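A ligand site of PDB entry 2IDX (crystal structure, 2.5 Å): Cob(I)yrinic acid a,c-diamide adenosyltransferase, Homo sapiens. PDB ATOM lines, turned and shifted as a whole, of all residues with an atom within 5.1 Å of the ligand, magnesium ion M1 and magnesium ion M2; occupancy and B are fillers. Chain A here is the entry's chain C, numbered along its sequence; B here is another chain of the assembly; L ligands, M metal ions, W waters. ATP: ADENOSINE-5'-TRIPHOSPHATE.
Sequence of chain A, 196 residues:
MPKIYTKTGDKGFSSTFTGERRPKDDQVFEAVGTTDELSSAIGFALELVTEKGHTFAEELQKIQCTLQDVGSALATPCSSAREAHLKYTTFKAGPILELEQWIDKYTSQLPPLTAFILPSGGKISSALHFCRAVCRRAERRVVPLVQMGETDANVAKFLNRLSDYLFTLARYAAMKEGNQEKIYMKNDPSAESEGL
Magnesium ion M1 is bound by OD1 of Asn 160 of chain B (2.0 Å), O2A of the ligand (2.0 Å), water W1 (2.1 Å), O3G of the ligand (2.1 Å), O2B of the ligand (2.2 Å) and water W4 (2.3 Å). Magnesium ion M1 has six donor atoms within binding distance.
ND2 of Asn 160 of chain B lies close to NZ of Lys 24 (3.4 Å). The backbone carbonyl oxygen (O) of Phe 29 sits at hydrogen-bond distance from the guanidinium group (NE) of Arg 140 of chain B, at 3.5 Å. NZ of Lys 24 sits at hydrogen-bond distance from O of Gly 9 (3.1 Å). The guanidinium group (NH1) of Arg 21 lies within hydrogen-bond range of the side-chain hydroxyl (OG) of Ser 15. The side-chain amide nitrogen (ND2) of Asn 160 of chain B is in hydrogen-bond range of the side-chain carboxylate (OD1) of Asp 10, at 3.1 Å. O of Arg 136 of chain B lies close to NH1 of Arg 140 of chain B (3.4 Å). OD1 of Asn 160 of chain B lies close to OE1 of Glu 139 of chain B (3.5 Å). The side-chain amino group (NZ) of Lys 24 lies within salt-bridge range of the side-chain carboxylate (OE1) of Glu 139 of chain B.
Water W4 lies within hydrogen-bond range of OE2 of Glu 139 of chain B (2.7 Å), N7 of the ligand (2.9 Å) and NZ of Lys 24 (3.0 Å). Water W1 lies within hydrogen-bond range of the side-chain carboxylate of Asp 164 of chain B (2.9 Å) and the side-chain hydroxyl of Ser 163 of chain B (3.0 Å). Water W6 lies within hydrogen-bond range of the side-chain carboxylate (OD1) of Asp 164 of chain B (2.8 Å) and an oxygen (O2G) of the ligand (3.2 Å). Water W5 bridges the backbone NH (N) of Thr 8 (2.6 Å) and an oxygen (O2G) of the ligand (2.7 Å). Water W8 lies within hydrogen-bond range of NH1 of Arg 21 (2.6 Å), OG1 of Thr 8 (2.7 Å), O1B of the ligand (3.1 Å) and N of Gly 9 (3.5 Å).
No residue comes within 4 Å of magnesium ion M2. The nearest printed residue that does not touch magnesium ion M2 is Asp 164 of chain B (4.04 Å).
NZ of Lys 24 touches magnesium ion M1, at 3.9 Å. Of the 20 residues printed, 2 come within 4 Å of magnesium ion M1.
Magnesium ion M2 is bound by water W2 (2.0 Å), water W7 (2.0 Å), water W6 (2.1 Å), an oxygen (O1A) of the ligand (2.1 Å) and water W3 (2.3 Å).
CB of Lys 7 touches O1G of the ligand, at 3.2 Å. Thr 8 touches the ligand. O of Phe 13 touches O1B of the ligand (3.7 Å). Phe 29 touches the ligand (O to C2, 3.3 Å). Gly 33 touches the ligand. Hydrophobic or aromatic side chains within 4 Å of the ligand: Phe 29. Within 4 Å of the ligand: Lys 7, Thr 8, Gly 9, Phe 13, Ser 14, Ser 15, Lys 24, Phe 29, Gly 33, Arg 136 of chain B, Glu 139 of chain B, Arg 140 of chain B and Asn 160 of chain B.
N of Gly 9 lies within hydrogen-bond range of O1G of the ligand. The backbone carbonyl oxygen of Arg 136 of chain B lies within hydrogen-bond range of a nitrogen (N6) of the ligand, at 3.1 Å. O of Ser 15 sits at hydrogen-bond distance from O2' of the ligand, at 2.8 Å. N6 of the ligand sits at hydrogen-bond distance from OE2 of Glu 139 of chain B, at 3.2 Å. NH1 of Arg 140 of chain B sits at hydrogen-bond distance from N1 of the ligand (2.8 Å). The side-chain amino group of Lys 24 lies close to an oxygen (O2B) of the ligand, at 2.6 Å. The guanidinium group (NH2) of Arg 136 of chain B sits close to an oxygen (O4') of the ligand. The side-chain hydroxyl (OG) of Ser 14 lies within hydrogen-bond range of an oxygen (O1B) of the ligand (2.9 Å).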
ATOM      1  N   LYS A   7      11.792   5.913   7.892  1.00  0.00           N
ATOM      2  CA  LYS A   7      10.710   6.877   7.777  1.00  0.00           C
ATOM      3  C   LYS A   7      11.250   8.056   7.000  1.00  0.00           C
ATOM      4  O   LYS A   7      12.441   8.388   7.074  1.00  0.00           O
ATOM      5  CB  LYS A   7      10.204   7.298   9.158  1.00  0.00           C
ATOM      6  CG  LYS A   7       9.670   6.152  10.011  1.00  0.00           C
ATOM      7  CD  LYS A   7       8.258   5.748   9.635  1.00  0.00           C
ATOM      8  CE  LYS A   7       7.636   4.940  10.749  1.00  0.00           C
ATOM      9  NZ  LYS A   7       6.376   4.213  10.377  1.00  0.00           N
ATOM     10  N   THR A   8      10.372   8.679   6.224  1.00  0.00           N
ATOM     11  CA  THR A   8      10.788   9.724   5.292  1.00  0.00           C
ATOM     12  C   THR A   8      11.343  10.949   6.019  1.00  0.00           C
ATOM     13  O   THR A   8      12.144  11.688   5.468  1.00  0.00           O
ATOM     14  CB  THR A   8       9.660  10.106   4.340  1.00  0.00           C
ATOM     15  OG1 THR A   8       8.519  10.484   5.107  1.00  0.00           O
ATOM     16  CG2 THR A   8       9.306   8.926   3.421  1.00  0.00           C
ATOM     17  N   GLY A   9      10.924  11.125   7.276  1.00  0.00           N
ATOM     18  CA  GLY A   9      11.362  12.235   8.117  1.00  0.00           C
ATOM     19  C   GLY A   9      12.659  12.045   8.873  1.00  0.00           C
ATOM     20  O   GLY A   9      13.168  12.980   9.485  1.00  0.00           O
ATOM     21  N   ASP A  10      13.214  10.837   8.814  1.00  0.00           N
ATOM     22  CA  ASP A  10      14.378  10.443   9.617  1.00  0.00           C
ATOM     23  C   ASP A  10      15.708  11.157   9.332  1.00  0.00           C
ATOM     24  O   ASP A  10      16.569  11.223  10.217  1.00  0.00           O
ATOM     25  CB  ASP A  10      14.576   8.929   9.547  1.00  0.00           C
ATOM     26  CG  ASP A  10      13.810   8.190  10.606  1.00  0.00           C
ATOM     27  OD1 ASP A  10      12.989   8.806  11.329  1.00  0.00           O
ATOM     28  OD2 ASP A  10      14.047   6.973  10.724  1.00  0.00           O
ATOM     29  N   PHE A  13      14.204  15.977   7.073  1.00  0.00           N
ATOM     30  CA  PHE A  13      13.446  16.706   6.038  1.00  0.00           C
ATOM     31  C   PHE A  13      11.959  16.322   6.117  1.00  0.00           C
ATOM     32  O   PHE A  13      11.612  15.208   6.530  1.00  0.00           O
ATOM     33  CB  PHE A  13      13.978  16.386   4.625  1.00  0.00           C
ATOM     34  CG  PHE A  13      15.349  16.925   4.373  1.00  0.00           C
ATOM     35  CD1 PHE A  13      16.477  16.209   4.758  1.00  0.00           C
ATOM     36  CD2 PHE A  13      15.521  18.156   3.738  1.00  0.00           C
ATOM     37  CE1 PHE A  13      17.760  16.708   4.539  1.00  0.00           C
ATOM     38  CE2 PHE A  13      16.794  18.676   3.497  1.00  0.00           C
ATOM     39  CZ  PHE A  13      17.931  17.955   3.892  1.00  0.00           C
ATOM     40  N   SER A  14      11.103  17.250   5.721  1.00  0.00           N
ATOM     41  CA  SER A  14       9.670  16.987   5.644  1.00  0.00           C
ATOM     42  C   SER A  14       9.104  17.662   4.403  1.00  0.00           C
ATOM     43  O   SER A  14       9.838  18.326   3.673  1.00  0.00           O
ATOM     44  CB  SER A  14       8.973  17.480   6.910  1.00  0.00           C
ATOM     45  OG  SER A  14       7.827  16.715   7.190  1.00  0.00           O
ATOM     46  N   SER A  15       7.801  17.501   4.160  1.00  0.00           N
ATOM     47  CA  SER A  15       7.174  18.062   2.969  1.00  0.00           C
ATOM     48  C   SER A  15       6.159  19.149   3.260  1.00  0.00           C
ATOM     49  O   SER A  15       5.494  19.110   4.309  1.00  0.00           O
ATOM     50  CB  SER A  15       6.468  16.966   2.151  1.00  0.00           C
ATOM     51  OG  SER A  15       7.417  16.122   1.539  1.00  0.00           O
ATOM     52  N   THR A  16       6.016  20.097   2.331  1.00  0.00           N
ATOM     53  CA  THR A  16       4.918  21.060   2.348  1.00  0.00           C
ATOM     54  C   THR A  16       3.761  20.437   1.582  1.00  0.00           C
ATOM     55  O   THR A  16       3.931  19.412   0.917  1.00  0.00           O
ATOM     56  CB  THR A  16       5.295  22.393   1.676  1.00  0.00           C
ATOM     57  OG1 THR A  16       5.477  22.212   0.254  1.00  0.00           O
ATOM     58  CG2 THR A  16       6.564  22.963   2.271  1.00  0.00           C
ATOM     59  N   ARG A  21      10.399  19.788  -0.477  1.00  0.00           N
ATOM     60  CA  ARG A  21      11.113  19.138   0.612  1.00  0.00           C
ATOM     61  C   ARG A  21      11.987  20.171   1.327  1.00  0.00           C
ATOM     62  O   ARG A  21      12.826  20.824   0.711  1.00  0.00           O
ATOM     63  CB  ARG A  21      12.011  18.017   0.067  1.00  0.00           C
ATOM     64  CG  ARG A  21      11.260  16.838  -0.562  1.00  0.00           C
ATOM     65  CD  ARG A  21      10.430  16.058   0.462  1.00  0.00           C
ATOM     66  NE  ARG A  21      11.281  15.336   1.422  1.00  0.00           N
ATOM     67  CZ  ARG A  21      10.828  14.686   2.491  1.00  0.00           C
ATOM     68  NH1 ARG A  21       9.519  14.674   2.771  1.00  0.00           N
ATOM     69  NH2 ARG A  21      11.675  14.058   3.294  1.00  0.00           N
ATOM     70  N   LYS A  24      13.485  20.256   8.588  1.00  0.00           N
ATOM     71  CA  LYS A  24      12.365  20.367   9.515  1.00  0.00           C
ATOM     72  C   LYS A  24      12.448  21.654  10.300  1.00  0.00           C
ATOM     73  O   LYS A  24      11.479  22.173  10.786  1.00  0.00           O
ATOM     74  CB  LYS A  24      12.321  19.133  10.437  1.00  0.00           C
ATOM     75  CG  LYS A  24      11.716  17.934   9.730  1.00  0.00           C
ATOM     76  CD  LYS A  24      11.658  16.704  10.626  1.00  0.00           C
ATOM     77  CE  LYS A  24      10.946  15.575   9.913  1.00  0.00           C
ATOM     78  NZ  LYS A  24      10.766  14.390  10.772  1.00  0.00           N
ATOM     79  N   PHE A  29       7.591  24.884   9.207  1.00  0.00           N
ATOM     80  CA  PHE A  29       7.330  23.891  10.219  1.00  0.00           C
ATOM     81  C   PHE A  29       7.414  24.492  11.623  1.00  0.00           C
ATOM     82  O   PHE A  29       6.779  24.016  12.562  1.00  0.00           O
ATOM     83  CB  PHE A  29       8.331  22.755  10.095  1.00  0.00           C
ATOM     84  CG  PHE A  29       8.399  22.157   8.725  1.00  0.00           C
ATOM     85  CD1 PHE A  29       9.604  22.146   8.025  1.00  0.00           C
ATOM     86  CD2 PHE A  29       7.277  21.622   8.123  1.00  0.00           C
ATOM     87  CE1 PHE A  29       9.674  21.587   6.738  1.00  0.00           C
ATOM     88  CE2 PHE A  29       7.351  21.057   6.829  1.00  0.00           C
ATOM     89  CZ  PHE A  29       8.552  21.036   6.148  1.00  0.00           C
ATOM     90  N   VAL A  32       3.905  25.891  11.627  1.00  0.00           N
ATOM     91  CA  VAL A  32       2.811  24.938  11.858  1.00  0.00           C
ATOM     92  C   VAL A  32       2.928  24.218  13.183  1.00  0.00           C
ATOM     93  O   VAL A  32       1.928  23.999  13.875  1.00  0.00           O
ATOM     94  CB  VAL A  32       2.440  23.973  10.628  1.00  0.00           C
ATOM     95  CG1 VAL A  32       3.289  24.186   9.391  1.00  0.00           C
ATOM     96  CG2 VAL A  32       2.345  22.493  11.052  1.00  0.00           C
ATOM     97  N   GLY A  33       4.149  23.870  13.554  1.00  0.00           N
ATOM     98  CA  GLY A  33       4.390  23.268  14.864  1.00  0.00           C
ATOM     99  C   GLY A  33       3.811  24.110  16.007  1.00  0.00           C
ATOM    100  O   GLY A  33       3.139  23.587  16.903  1.00  0.00           O
ATOM    101  N   ARG B 136       7.724  17.689  18.880  1.00  0.00           N
ATOM    102  CA  ARG B 136       8.001  18.110  17.518  1.00  0.00           C
ATOM    103  C   ARG B 136       8.857  19.410  17.464  1.00  0.00           C
ATOM    104  O   ARG B 136       9.690  19.607  16.550  1.00  0.00           O
ATOM    105  CB  ARG B 136       6.695  18.232  16.724  1.00  0.00           C
ATOM    106  CG  ARG B 136       6.056  16.880  16.474  1.00  0.00           C
ATOM    107  CD  ARG B 136       4.601  16.916  16.032  1.00  0.00           C
ATOM    108  NE  ARG B 136       4.458  17.435  14.677  1.00  0.00           N
ATOM    109  CZ  ARG B 136       4.572  16.713  13.554  1.00  0.00           C
ATOM    110  NH1 ARG B 136       4.835  15.421  13.605  1.00  0.00           N
ATOM    111  NH2 ARG B 136       4.432  17.294  12.376  1.00  0.00           N
ATOM    112  N   ARG B 137       8.659  20.280  18.453  1.00  0.00           N
ATOM    113  CA  ARG B 137       9.505  21.457  18.585  1.00  0.00           C
ATOM    114  C   ARG B 137      10.940  21.013  18.907  1.00  0.00           C
ATOM    115  O   ARG B 137      11.899  21.598  18.413  1.00  0.00           O
ATOM    116  CB  ARG B 137       8.942  22.399  19.661  1.00  0.00           C
ATOM    117  CG  ARG B 137       9.472  23.798  19.629  1.00  0.00           C
ATOM    118  CD  ARG B 137       8.581  24.733  20.457  1.00  0.00           C
ATOM    119  NE  ARG B 137       9.144  24.819  21.802  1.00  0.00           N
ATOM    120  CZ  ARG B 137       8.499  24.637  22.943  1.00  0.00           C
ATOM    121  NH1 ARG B 137       7.200  24.435  23.025  1.00  0.00           N
ATOM    122  NH2 ARG B 137       9.195  24.705  24.032  1.00  0.00           N
ATOM    123  N   GLU B 139      12.353  18.242  18.056  1.00  0.00           N
ATOM    124  CA  GLU B 139      12.862  17.706  16.821  1.00  0.00           C
ATOM    125  C   GLU B 139      13.409  18.798  15.947  1.00  0.00           C
ATOM    126  O   GLU B 139      14.585  18.738  15.545  1.00  0.00           O
ATOM    127  CB  GLU B 139      11.804  16.912  16.078  1.00  0.00           C
ATOM    128  CG  GLU B 139      12.359  16.210  14.856  1.00  0.00           C
ATOM    129  CD  GLU B 139      11.282  15.459  14.069  1.00  0.00           C
ATOM    130  OE1 GLU B 139      11.656  14.679  13.160  1.00  0.00           O
ATOM    131  OE2 GLU B 139      10.085  15.611  14.362  1.00  0.00           O
ATOM    132  N   ARG B 140      12.604  19.816  15.667  1.00  0.00           N
ATOM    133  CA  ARG B 140      13.089  20.935  14.846  1.00  0.00           C
ATOM    134  C   ARG B 140      14.380  21.547  15.380  1.00  0.00           C
ATOM    135  O   ARG B 140      15.180  22.034  14.616  1.00  0.00           O
ATOM    136  CB  ARG B 140      12.014  22.012  14.650  1.00  0.00           C
ATOM    137  CG  ARG B 140      10.748  21.484  14.011  1.00  0.00           C
ATOM    138  CD  ARG B 140       9.775  22.567  13.622  1.00  0.00           C
ATOM    139  NE  ARG B 140       9.419  23.465  14.717  1.00  0.00           N
ATOM    140  CZ  ARG B 140       8.432  23.251  15.580  1.00  0.00           C
ATOM    141  NH1 ARG B 140       7.694  22.143  15.517  1.00  0.00           N
ATOM    142  NH2 ARG B 140       8.188  24.147  16.521  1.00  0.00           N
ATOM    143  N   ASN B 160      11.701  12.072  16.135  1.00  0.00           N
ATOM    144  CA  ASN B 160      10.698  11.883  15.077  1.00  0.00           C
ATOM    145  C   ASN B 160       9.693  10.812  15.465  1.00  0.00           C
ATOM    146  O   ASN B 160       8.491  10.998  15.326  1.00  0.00           O
ATOM    147  CB  ASN B 160      11.371  11.491  13.762  1.00  0.00           C
ATOM    148  CG  ASN B 160      10.427  11.564  12.569  1.00  0.00           C
ATOM    149  OD1 ASN B 160       9.323  12.138  12.654  1.00  0.00           O
ATOM    150  ND2 ASN B 160      10.858  11.008  11.441  1.00  0.00           N
ATOM    151  N   SER B 163       7.120  11.496  18.617  1.00  0.00           N
ATOM    152  CA  SER B 163       5.826  12.151  18.402  1.00  0.00           C
ATOM    153  C   SER B 163       4.760  11.194  17.873  1.00  0.00           C
ATOM    154  O   SER B 163       3.558  11.391  18.143  1.00  0.00           O
ATOM    155  CB  SER B 163       5.916  13.432  17.555  1.00  0.00           C
ATOM    156  OG  SER B 163       6.212  13.201  16.197  1.00  0.00           O
ATOM    157  N   ASP B 164       5.179  10.153  17.148  1.00  0.00           N
ATOM    158  CA  ASP B 164       4.241   9.094  16.746  1.00  0.00           C
ATOM    159  C   ASP B 164       3.823   8.323  17.969  1.00  0.00           C
ATOM    160  O   ASP B 164       2.655   8.003  18.122  1.00  0.00           O
ATOM    161  CB  ASP B 164       4.849   8.142  15.705  1.00  0.00           C
ATOM    162  CG  ASP B 164       5.149   8.828  14.392  1.00  0.00           C
ATOM    163  OD1 ASP B 164       4.559   9.897  14.090  1.00  0.00           O
ATOM    164  OD2 ASP B 164       5.997   8.305  13.642  1.00  0.00           O
HETATM  165  PG  ATP L   1       7.618  10.543   9.374  1.00  0.00           P
HETATM  166  O1G ATP L   1       9.090  10.348   9.182  1.00  0.00           O
HETATM  167  O2G ATP L   1       6.646   9.513   8.862  1.00  0.00           O
HETATM  168  O3G ATP L   1       7.269  10.992  10.786  1.00  0.00           O
HETATM  169  PB  ATP L   1       7.655  13.382   8.832  1.00  0.00           P
HETATM  170  O1B ATP L   1       8.337  13.921   7.596  1.00  0.00           O
HETATM  171  O2B ATP L   1       8.333  13.582  10.159  1.00  0.00           O
HETATM  172  O3B ATP L   1       7.327  11.836   8.471  1.00  0.00           O
HETATM  173  PA  ATP L   1       5.128  13.618  10.071  1.00  0.00           P
HETATM  174  O1A ATP L   1       4.131  12.604   9.614  1.00  0.00           O
HETATM  175  O2A ATP L   1       5.865  13.406  11.369  1.00  0.00           O
HETATM  176  O3A ATP L   1       6.148  13.944   8.878  1.00  0.00           O
HETATM  177  O5' ATP L   1       4.367  15.039  10.151  1.00  0.00           O
HETATM  178  C5' ATP L   1       3.213  15.375   9.370  1.00  0.00           C
HETATM  179  C4' ATP L   1       3.499  16.702   8.676  1.00  0.00           C
HETATM  180  O4' ATP L   1       3.811  17.674   9.671  1.00  0.00           O
HETATM  181  C3' ATP L   1       4.704  16.701   7.759  1.00  0.00           C
HETATM  182  O3' ATP L   1       4.374  16.426   6.392  1.00  0.00           O
HETATM  183  C2' ATP L   1       5.295  18.100   7.890  1.00  0.00           C
HETATM  184  O2' ATP L   1       4.697  19.026   7.009  1.00  0.00           O
HETATM  185  C1' ATP L   1       4.883  18.515   9.261  1.00  0.00           C
HETATM  186  N9  ATP L   1       5.979  18.243  10.208  1.00  0.00           N
HETATM  187  C8  ATP L   1       6.799  17.178  10.214  1.00  0.00           C
HETATM  188  N7  ATP L   1       7.685  17.264  11.223  1.00  0.00           N
HETATM  189  C5  ATP L   1       7.390  18.396  11.899  1.00  0.00           C
HETATM  190  C6  ATP L   1       7.930  19.078  13.084  1.00  0.00           C
HETATM  191  N6  ATP L   1       8.980  18.543  13.773  1.00  0.00           N
HETATM  192  N1  ATP L   1       7.337  20.258  13.420  1.00  0.00           N
HETATM  193  C2  ATP L   1       6.306  20.797  12.768  1.00  0.00           C
HETATM  194  N3  ATP L   1       5.759  20.216  11.697  1.00  0.00           N
HETATM  195  C4  ATP L   1       6.269  19.042  11.224  1.00  0.00           C
HETATM  196 MG    MG M   1       7.541  12.655  12.041  1.00  0.00          MG
HETATM  197 MG    MG M   2       3.093  10.931  10.466  1.00  0.00          MG
HETATM  198  O   HOH W   1       6.856  11.639  13.706  1.00  0.00           O
HETATM  199  O   HOH W   2       1.801   9.451  10.379  1.00  0.00           O
HETATM  200  O   HOH W   3       4.280  10.102   8.719  1.00  0.00           O
HETATM  201  O   HOH W   4       8.380  14.708  12.492  1.00  0.00           O
HETATM  202  O   HOH W   5       7.807   8.267   6.720  1.00  0.00           O
HETATM  203  O   HOH W   6       4.930  10.477  11.357  1.00  0.00           O
HETATM  204  O   HOH W   7       1.867  11.737   9.133  1.00  0.00           O
HETATM  205  O   HOH W   8       9.381  13.066   4.851  1.00  0.00           O
